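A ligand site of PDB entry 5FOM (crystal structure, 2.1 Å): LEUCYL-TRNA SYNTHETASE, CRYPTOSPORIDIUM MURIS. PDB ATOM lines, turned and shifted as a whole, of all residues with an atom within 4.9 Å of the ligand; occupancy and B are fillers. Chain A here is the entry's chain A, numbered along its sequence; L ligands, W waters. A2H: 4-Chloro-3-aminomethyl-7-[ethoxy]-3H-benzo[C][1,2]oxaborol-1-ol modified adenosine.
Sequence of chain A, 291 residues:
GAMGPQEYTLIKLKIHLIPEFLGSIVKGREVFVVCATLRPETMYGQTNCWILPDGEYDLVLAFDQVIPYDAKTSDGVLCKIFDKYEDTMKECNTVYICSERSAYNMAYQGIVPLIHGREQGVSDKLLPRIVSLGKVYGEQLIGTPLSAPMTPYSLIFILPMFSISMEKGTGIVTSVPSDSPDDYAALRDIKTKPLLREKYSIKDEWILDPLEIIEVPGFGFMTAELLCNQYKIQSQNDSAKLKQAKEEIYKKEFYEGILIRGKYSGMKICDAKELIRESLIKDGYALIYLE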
ATOM      1  N   GLN A   6       9.237   9.920   1.847  1.00  0.00           N
ATOM      2  CA  GLN A   6       9.057  11.355   2.039  1.00  0.00           C
ATOM      3  C   GLN A   6      10.409  12.046   1.844  1.00  0.00           C
ATOM      4  O   GLN A   6      11.444  11.523   2.241  1.00  0.00           O
ATOM      5  CB  GLN A   6       8.540  11.650   3.443  1.00  0.00           C
ATOM      6  CG  GLN A   6       7.656  10.556   4.041  1.00  0.00           C
ATOM      7  CD  GLN A   6       6.823  11.079   5.190  1.00  0.00           C
ATOM      8  OE1 GLN A   6       5.996  11.962   5.000  1.00  0.00           O
ATOM      9  NE2 GLN A   6       7.062  10.555   6.377  1.00  0.00           N
ATOM     10  N   TYR A   8      12.905  15.350   2.476  1.00  0.00           N
ATOM     11  CA  TYR A   8      13.264  16.362   3.443  1.00  0.00           C
ATOM     12  C   TYR A   8      14.482  17.152   2.966  1.00  0.00           C
ATOM     13  O   TYR A   8      15.171  16.760   1.997  1.00  0.00           O
ATOM     14  CB  TYR A   8      13.598  15.696   4.781  1.00  0.00           C
ATOM     15  CG  TYR A   8      12.433  14.946   5.387  1.00  0.00           C
ATOM     16  CD1 TYR A   8      11.440  15.622   6.102  1.00  0.00           C
ATOM     17  CD2 TYR A   8      12.312  13.558   5.256  1.00  0.00           C
ATOM     18  CE1 TYR A   8      10.361  14.935   6.660  1.00  0.00           C
ATOM     19  CE2 TYR A   8      11.224  12.866   5.813  1.00  0.00           C
ATOM     20  CZ  TYR A   8      10.260  13.574   6.513  1.00  0.00           C
ATOM     21  OH  TYR A   8       9.169  12.940   7.080  1.00  0.00           O
ATOM     22  N   ALA A  36      16.619  17.048  10.092  1.00  0.00           N
ATOM     23  CA  ALA A  36      15.671  16.950   8.976  1.00  0.00           C
ATOM     24  C   ALA A  36      14.570  17.994   9.171  1.00  0.00           C
ATOM     25  O   ALA A  36      14.077  18.178  10.294  1.00  0.00           O
ATOM     26  CB  ALA A  36      15.077  15.546   8.881  1.00  0.00           C
ATOM     27  N   THR A  37      14.223  18.719   8.106  1.00  0.00           N
ATOM     28  CA  THR A  37      13.136  19.698   8.148  1.00  0.00           C
ATOM     29  C   THR A  37      12.307  19.588   6.902  1.00  0.00           C
ATOM     30  O   THR A  37      12.822  19.266   5.828  1.00  0.00           O
ATOM     31  CB  THR A  37      13.638  21.144   8.278  1.00  0.00           C
ATOM     32  OG1 THR A  37      12.508  22.013   8.463  1.00  0.00           O
ATOM     33  CG2 THR A  37      14.409  21.599   7.015  1.00  0.00           C
ATOM     34  N   LEU A  38      11.020  19.851   7.053  1.00  0.00           N
ATOM     35  CA  LEU A  38      10.123  20.033   5.904  1.00  0.00           C
ATOM     36  C   LEU A  38      10.120  21.477   5.433  1.00  0.00           C
ATOM     37  O   LEU A  38       9.491  21.757   4.408  1.00  0.00           O
ATOM     38  CB  LEU A  38       8.688  19.656   6.291  1.00  0.00           C
ATOM     39  CG  LEU A  38       8.393  18.188   6.416  1.00  0.00           C
ATOM     40  CD1 LEU A  38       7.064  17.990   7.129  1.00  0.00           C
ATOM     41  CD2 LEU A  38       8.372  17.531   5.050  1.00  0.00           C
ATOM     42  N   ARG A  39      10.756  22.402   6.180  1.00  0.00           N
ATOM     43  CA  ARG A  39      10.589  23.846   5.958  1.00  0.00           C
ATOM     44  C   ARG A  39      11.919  24.600   5.895  1.00  0.00           C
ATOM     45  O   ARG A  39      12.316  25.313   6.844  1.00  0.00           O
ATOM     46  CB  ARG A  39       9.669  24.408   7.031  1.00  0.00           C
ATOM     47  CG  ARG A  39       8.293  23.709   7.001  1.00  0.00           C
ATOM     48  CD  ARG A  39       7.241  24.516   7.706  1.00  0.00           C
ATOM     49  NE  ARG A  39       7.021  25.795   7.059  1.00  0.00           N
ATOM     50  CZ  ARG A  39       6.473  26.871   7.618  1.00  0.00           C
ATOM     51  NH1 ARG A  39       6.048  26.861   8.893  1.00  0.00           N
ATOM     52  NH2 ARG A  39       6.360  27.977   6.906  1.00  0.00           N
ATOM     53  N   THR A  42      12.172  28.471   6.642  1.00  0.00           N
ATOM     54  CA  THR A  42      12.072  29.002   7.995  1.00  0.00           C
ATOM     55  C   THR A  42      13.419  29.120   8.719  1.00  0.00           C
ATOM     56  O   THR A  42      13.455  29.516   9.870  1.00  0.00           O
ATOM     57  CB  THR A  42      11.163  28.085   8.834  1.00  0.00           C
ATOM     58  OG1 THR A  42      11.732  26.776   8.875  1.00  0.00           O
ATOM     59  CG2 THR A  42       9.781  28.038   8.212  1.00  0.00           C
ATOM     60  N   SER A 163       9.479  15.419  22.949  1.00  0.00           N
ATOM     61  CA  SER A 163       8.595  14.866  21.922  1.00  0.00           C
ATOM     62  C   SER A 163       9.325  14.234  20.722  1.00  0.00           C
ATOM     63  O   SER A 163       8.666  13.650  19.858  1.00  0.00           O
ATOM     64  CB  SER A 163       7.621  15.959  21.459  1.00  0.00           C
ATOM     65  OG  SER A 163       8.295  17.203  21.358  1.00  0.00           O
ATOM     66  N   ILE A 164      10.652  14.362  20.635  1.00  0.00           N
ATOM     67  CA  ILE A 164      11.433  13.829  19.483  1.00  0.00           C
ATOM     68  C   ILE A 164      11.340  12.299  19.370  1.00  0.00           C
ATOM     69  O   ILE A 164      11.652  11.615  20.329  1.00  0.00           O
ATOM     70  CB  ILE A 164      12.928  14.233  19.589  1.00  0.00           C
ATOM     71  CG1 ILE A 164      13.083  15.698  19.186  1.00  0.00           C
ATOM     72  CG2 ILE A 164      13.815  13.370  18.688  1.00  0.00           C
ATOM     73  CD1 ILE A 164      14.397  16.326  19.577  1.00  0.00           C
ATOM     74  N   SER A 165      10.892  11.801  18.211  1.00  0.00           N
ATOM     75  CA  SER A 165      10.962  10.366  17.854  1.00  0.00           C
ATOM     76  C   SER A 165      12.312  10.013  17.212  1.00  0.00           C
ATOM     77  O   SER A 165      12.694  10.598  16.183  1.00  0.00           O
ATOM     78  CB  SER A 165       9.840  10.025  16.876  1.00  0.00           C
ATOM     79  OG  SER A 165       9.979   8.720  16.360  1.00  0.00           O
ATOM     80  N   LYS A 168      12.253   8.833  13.335  1.00  0.00           N
ATOM     81  CA  LYS A 168      12.020   9.794  12.251  1.00  0.00           C
ATOM     82  C   LYS A 168      13.227  10.693  12.046  1.00  0.00           C
ATOM     83  O   LYS A 168      13.889  11.052  12.984  1.00  0.00           O
ATOM     84  CB  LYS A 168      10.839  10.690  12.591  1.00  0.00           C
ATOM     85  CG  LYS A 168       9.461  10.057  12.441  1.00  0.00           C
ATOM     86  CD  LYS A 168       8.389  11.114  12.263  1.00  0.00           C
ATOM     87  CE  LYS A 168       8.242  12.044  13.478  1.00  0.00           C
ATOM     88  NZ  LYS A 168       8.121  13.472  13.082  1.00  0.00           N
ATOM     89  N   GLY A 169      13.456  11.112  10.813  1.00  0.00           N
ATOM     90  CA  GLY A 169      14.553  12.039  10.498  1.00  0.00           C
ATOM     91  C   GLY A 169      15.851  11.557  11.061  1.00  0.00           C
ATOM     92  O   GLY A 169      16.150  10.377  10.985  1.00  0.00           O
ATOM     93  N   GLY A 171      16.583  12.286  14.374  1.00  0.00           N
ATOM     94  CA  GLY A 171      16.444  12.527  15.799  1.00  0.00           C
ATOM     95  C   GLY A 171      16.937  13.879  16.279  1.00  0.00           C
ATOM     96  O   GLY A 171      16.986  14.131  17.488  1.00  0.00           O
ATOM     97  N   ILE A 172      17.304  14.766  15.350  1.00  0.00           N
ATOM     98  CA  ILE A 172      17.730  16.117  15.706  1.00  0.00           C
ATOM     99  C   ILE A 172      16.922  17.086  14.861  1.00  0.00           C
ATOM    100  O   ILE A 172      16.672  16.842  13.679  1.00  0.00           O
ATOM    101  CB  ILE A 172      19.237  16.312  15.564  1.00  0.00           C
ATOM    102  CG1 ILE A 172      20.000  15.112  16.146  1.00  0.00           C
ATOM    103  CG2 ILE A 172      19.657  17.589  16.233  1.00  0.00           C
ATOM    104  CD1 ILE A 172      21.521  15.196  16.078  1.00  0.00           C
ATOM    105  N   VAL A 173      16.461  18.159  15.503  1.00  0.00           N
ATOM    106  CA  VAL A 173      15.428  19.007  14.958  1.00  0.00           C
ATOM    107  C   VAL A 173      15.856  20.443  15.155  1.00  0.00           C
ATOM    108  O   VAL A 173      16.318  20.806  16.231  1.00  0.00           O
ATOM    109  CB  VAL A 173      14.057  18.750  15.640  1.00  0.00           C
ATOM    110  CG1 VAL A 173      12.968  19.638  15.058  1.00  0.00           C
ATOM    111  CG2 VAL A 173      13.630  17.278  15.517  1.00  0.00           C
ATOM    112  N   THR A 174      15.720  21.277  14.134  1.00  0.00           N
ATOM    113  CA  THR A 174      16.000  22.698  14.346  1.00  0.00           C
ATOM    114  C   THR A 174      14.760  23.407  14.876  1.00  0.00           C
ATOM    115  O   THR A 174      13.619  22.908  14.713  1.00  0.00           O
ATOM    116  CB  THR A 174      16.649  23.391  13.128  1.00  0.00           C
ATOM    117  OG1 THR A 174      17.282  24.623  13.582  1.00  0.00           O
ATOM    118  CG2 THR A 174      15.635  23.600  12.011  1.00  0.00           C
ATOM    119  N   SER A 175      15.003  24.529  15.555  1.00  0.00           N
ATOM    120  CA  SER A 175      13.956  25.224  16.312  1.00  0.00           C
ATOM    121  C   SER A 175      13.625  26.588  15.727  1.00  0.00           C
ATOM    122  O   SER A 175      14.467  27.462  15.701  1.00  0.00           O
ATOM    123  CB  SER A 175      14.353  25.364  17.785  1.00  0.00           C
ATOM    124  OG  SER A 175      13.299  25.921  18.539  1.00  0.00           O
ATOM    125  N   VAL A 176      12.398  26.720  15.241  1.00  0.00           N
ATOM    126  CA  VAL A 176      11.861  27.959  14.752  1.00  0.00           C
ATOM    127  C   VAL A 176      10.520  28.219  15.500  1.00  0.00           C
ATOM    128  O   VAL A 176       9.442  27.964  14.943  1.00  0.00           O
ATOM    129  CB  VAL A 176      11.624  27.894  13.235  1.00  0.00           C
ATOM    130  CG1 VAL A 176      11.217  29.271  12.722  1.00  0.00           C
ATOM    131  CG2 VAL A 176      12.872  27.400  12.516  1.00  0.00           C
ATOM    132  N   ASP A 179       7.090  29.967  14.088  1.00  0.00           N
ATOM    133  CA  ASP A 179       6.237  29.324  13.077  1.00  0.00           C
ATOM    134  C   ASP A 179       6.114  27.780  13.173  1.00  0.00           C
ATOM    135  O   ASP A 179       5.606  27.163  12.227  1.00  0.00           O
ATOM    136  CB  ASP A 179       6.697  29.749  11.689  1.00  0.00           C
ATOM    137  CG  ASP A 179       6.476  31.245  11.444  1.00  0.00           C
ATOM    138  OD1 ASP A 179       5.359  31.615  11.060  1.00  0.00           O
ATOM    139  OD2 ASP A 179       7.429  32.053  11.623  1.00  0.00           O
ATOM    140  N   SER A 180       6.565  27.201  14.286  1.00  0.00           N
ATOM    141  CA  SER A 180       6.377  25.785  14.615  1.00  0.00           C
ATOM    142  C   SER A 180       5.735  25.663  15.997  1.00  0.00           C
ATOM    143  O   SER A 180       6.346  26.052  16.990  1.00  0.00           O
ATOM    144  CB  SER A 180       7.698  25.022  14.645  1.00  0.00           C
ATOM    145  OG  SER A 180       7.536  23.749  15.262  1.00  0.00           O
ATOM    146  N   ASP A 183       7.961  23.784  18.391  1.00  0.00           N
ATOM    147  CA  ASP A 183       9.149  24.533  18.789  1.00  0.00           C
ATOM    148  C   ASP A 183       8.773  25.619  19.811  1.00  0.00           C
ATOM    149  O   ASP A 183       9.470  25.796  20.821  1.00  0.00           O
ATOM    150  CB  ASP A 183       9.849  25.162  17.583  1.00  0.00           C
ATOM    151  CG  ASP A 183      10.411  24.130  16.616  1.00  0.00           C
ATOM    152  OD1 ASP A 183      10.591  22.951  16.984  1.00  0.00           O
ATOM    153  OD2 ASP A 183      10.699  24.515  15.461  1.00  0.00           O
ATOM    154  N   LYS A 246      -0.216  21.840  13.821  1.00  0.00           N
ATOM    155  CA  LYS A 246       0.829  21.630  12.810  1.00  0.00           C
ATOM    156  C   LYS A 246       0.280  21.451  11.408  1.00  0.00           C
ATOM    157  O   LYS A 246       0.884  21.955  10.452  1.00  0.00           O
ATOM    158  CB  LYS A 246       1.703  20.416  13.160  1.00  0.00           C
ATOM    159  CG  LYS A 246       2.667  20.651  14.319  1.00  0.00           C
ATOM    160  CD  LYS A 246       3.979  19.890  14.136  1.00  0.00           C
ATOM    161  CE  LYS A 246       3.785  18.387  14.207  1.00  0.00           C
ATOM    162  NZ  LYS A 246       3.309  17.960  15.543  1.00  0.00           N
ATOM    163  N   TYR A 250       0.896  24.345   8.627  1.00  0.00           N
ATOM    164  CA  TYR A 250       1.697  23.911   7.471  1.00  0.00           C
ATOM    165  C   TYR A 250       1.080  24.397   6.167  1.00  0.00           C
ATOM    166  O   TYR A 250       1.783  25.020   5.335  1.00  0.00           O
ATOM    167  CB  TYR A 250       1.922  22.375   7.426  1.00  0.00           C
ATOM    168  CG  TYR A 250       2.947  22.001   6.367  1.00  0.00           C
ATOM    169  CD1 TYR A 250       4.310  21.976   6.662  1.00  0.00           C
ATOM    170  CD2 TYR A 250       2.561  21.737   5.046  1.00  0.00           C
ATOM    171  CE1 TYR A 250       5.256  21.671   5.683  1.00  0.00           C
ATOM    172  CE2 TYR A 250       3.493  21.435   4.067  1.00  0.00           C
ATOM    173  CZ  TYR A 250       4.842  21.408   4.392  1.00  0.00           C
ATOM    174  OH  TYR A 250       5.768  21.112   3.424  1.00  0.00           O
HETATM  175  B   A2H L   1      10.075  20.936  10.848  1.00  0.00           B
HETATM  176  P   A2H L   1       7.354  14.500   9.734  1.00  0.00           P
HETATM  177 CL   A2H L   1       9.151  25.984  11.283  1.00  0.00          CL
HETATM  178  N1  A2H L   1      10.972  14.051  16.010  1.00  0.00           N
HETATM  179  O1  A2H L   1      11.191  21.883  10.648  1.00  0.00           O
HETATM  180  C2  A2H L   1      10.051  15.025  16.086  1.00  0.00           C
HETATM  181  N3  A2H L   1       9.951  15.961  15.112  1.00  0.00           N
HETATM  182  C4  A2H L   1      10.797  15.941  14.046  1.00  0.00           C
HETATM  183  C5  A2H L   1      11.763  14.939  13.946  1.00  0.00           C
HETATM  184  C6  A2H L   1      11.837  13.983  14.946  1.00  0.00           C
HETATM  185  N6  A2H L   1      12.767  13.018  14.841  1.00  0.00           N
HETATM  186  N7  A2H L   1      12.464  15.125  12.799  1.00  0.00           N
HETATM  187  C8  A2H L   1      11.946  16.223  12.206  1.00  0.00           C
HETATM  188  N9  A2H L   1      10.945  16.718  12.962  1.00  0.00           N
HETATM  189  C1' A2H L   1      10.109  17.904  12.720  1.00  0.00           C
HETATM  190  C10 A2H L   1      10.858  23.234  10.964  1.00  0.00           C
HETATM  191  C11 A2H L   1       9.374  23.185  11.039  1.00  0.00           C
HETATM  192  C12 A2H L   1       8.896  21.885  10.923  1.00  0.00           C
HETATM  193  C13 A2H L   1       8.532  24.291  11.149  1.00  0.00           C
HETATM  194  C14 A2H L   1       7.155  24.066  11.178  1.00  0.00           C
HETATM  195  C15 A2H L   1       6.629  22.779  11.083  1.00  0.00           C
HETATM  196  C16 A2H L   1       7.491  21.666  10.952  1.00  0.00           C
HETATM  197  C17 A2H L   1      11.555  23.674  12.241  1.00  0.00           C
HETATM  198  N18 A2H L   1      11.303  22.746  13.308  1.00  0.00           N
HETATM  199  O19 A2H L   1       6.962  20.398  10.881  1.00  0.00           O
HETATM  200  O1P A2H L   1       8.480  13.747  10.379  1.00  0.00           O
HETATM  201  C2' A2H L   1      10.834  18.944  11.867  1.00  0.00           C
HETATM  202  O2' A2H L   1      10.373  20.276  12.065  1.00  0.00           O
HETATM  203  C20 A2H L   1       5.611  20.037  10.553  1.00  0.00           C
HETATM  204  C21 A2H L   1       5.360  18.591  10.966  1.00  0.00           C
HETATM  205  O2P A2H L   1       6.044  14.291  10.446  1.00  0.00           O
HETATM  206  C3' A2H L   1      10.417  18.636  10.456  1.00  0.00           C
HETATM  207  O3' A2H L   1      10.221  19.922   9.863  1.00  0.00           O
HETATM  208  O3P A2H L   1       7.296  14.492   8.220  1.00  0.00           O
HETATM  209  C4' A2H L   1       9.113  17.861  10.609  1.00  0.00           C
HETATM  210  O4' A2H L   1       8.978  17.508  11.987  1.00  0.00           O
HETATM  211  C5' A2H L   1       9.036  16.571   9.846  1.00  0.00           C
HETATM  212  O5' A2H L   1       7.739  16.032  10.068  1.00  0.00           O
HETATM  213  O   HOH W   1      13.935  20.589  11.804  1.00  0.00           O
HETATM  214  O   HOH W   2       7.270  19.897  13.513  1.00  0.00           O
HETATM  215  O   HOH W   3      15.386  14.986  12.244  1.00  0.00           O
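Ala 36 touches the ligand (O to C8, 3.5 Å).
CD of Arg 39 touches C14 of the ligand (3.5 Å).
OG1 of Thr 42 touches CL of the ligand, 3.6 Å away.
Ile 164 touches the ligand.
Gly 171 touches the ligand.
CG2 of Val 173 touches C5 of the ligand, at 3.4 Å.
Val 176 touches the ligand (CB to CL, 3.7 Å).
O of Asp 179 touches C14 of the ligand, at 3.6 Å.
CB of Ser 180 touches C14 of the ligand (3.6 Å).
CE of Lys 246 touches C21 of the ligand (3.6 Å).
Hydrophobic or aromatic side chains that line the ligand: Tyr 8, Leu 38, Ile 164, Val 173 and Val 176.
The nearest printed residue that does not touch the ligand is Ser 163 (4.2 Å).
The side-chain hydroxyl (OG1) of Thr 37 sits at hydrogen-bond distance from an oxygen (O1) of the ligand (2.6 Å).
The side-chain hydroxyl (OH) of Tyr 8 lies within hydrogen-bond range of an oxygen (O3P) of the ligand, at 2.7 Å.
A nitrogen (N18) of the ligand sits at hydrogen-bond distance from the backbone carbonyl oxygen (O) of Thr 174.
The backbone carbonyl oxygen of Lys 168 lies within hydrogen-bond range of a nitrogen (N6) of the ligand (2.9 Å).
NZ of Lys 168 is in salt-bridge range of O1P of the ligand (2.7 Å).
A nitrogen (N1) of the ligand lies within hydrogen-bond range of the backbone NH (N) of Ser 165.
A nitrogen (N6) of the ligand sits at hydrogen-bond distance from the backbone carbonyl oxygen of Ser 165 (2.8 Å).
A nitrogen (N18) of the ligand lies within salt-bridge range of the side-chain carboxylate (OD2) of Asp 183, 2.9 Å away.
The backbone NH of Leu 38 is in hydrogen-bond range of an oxygen (O3') of the ligand (2.9 Å).
OG1 of Thr 37 lies within hydrogen-bond range of N of Arg 39, at 2.9 Å.
The side-chain hydroxyl (OH) of Tyr 8 sits at hydrogen-bond distance from the side-chain amide nitrogen (NE2) of Gln 6.
The backbone NH (N) of Asp 183 sits at hydrogen-bond distance from the side-chain hydroxyl (OG) of Ser 180 (3.2 Å).
The side-chain carboxylate (OD2) of Asp 183 sits at hydrogen-bond distance from the backbone NH (N) of Val 176, 2.8 Å away.
The backbone carbonyl oxygen (O) of Asp 179 sits at hydrogen-bond distance from the guanidinium group (NH1) of Arg 39.
O of Arg 39 is in hydrogen-bond range of OG1 of Thr 42 (2.6 Å).
Water W3 lies within hydrogen-bond range of O of Ile 172 (2.7 Å), N7 of the ligand (3.0 Å) and N of Ala 36 (3.2 Å).
Water W1 lies within hydrogen-bond range of O of Ala 36 (2.8 Å), N of Thr 174 (3.0 Å) and O1 of the ligand (3.2 Å).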
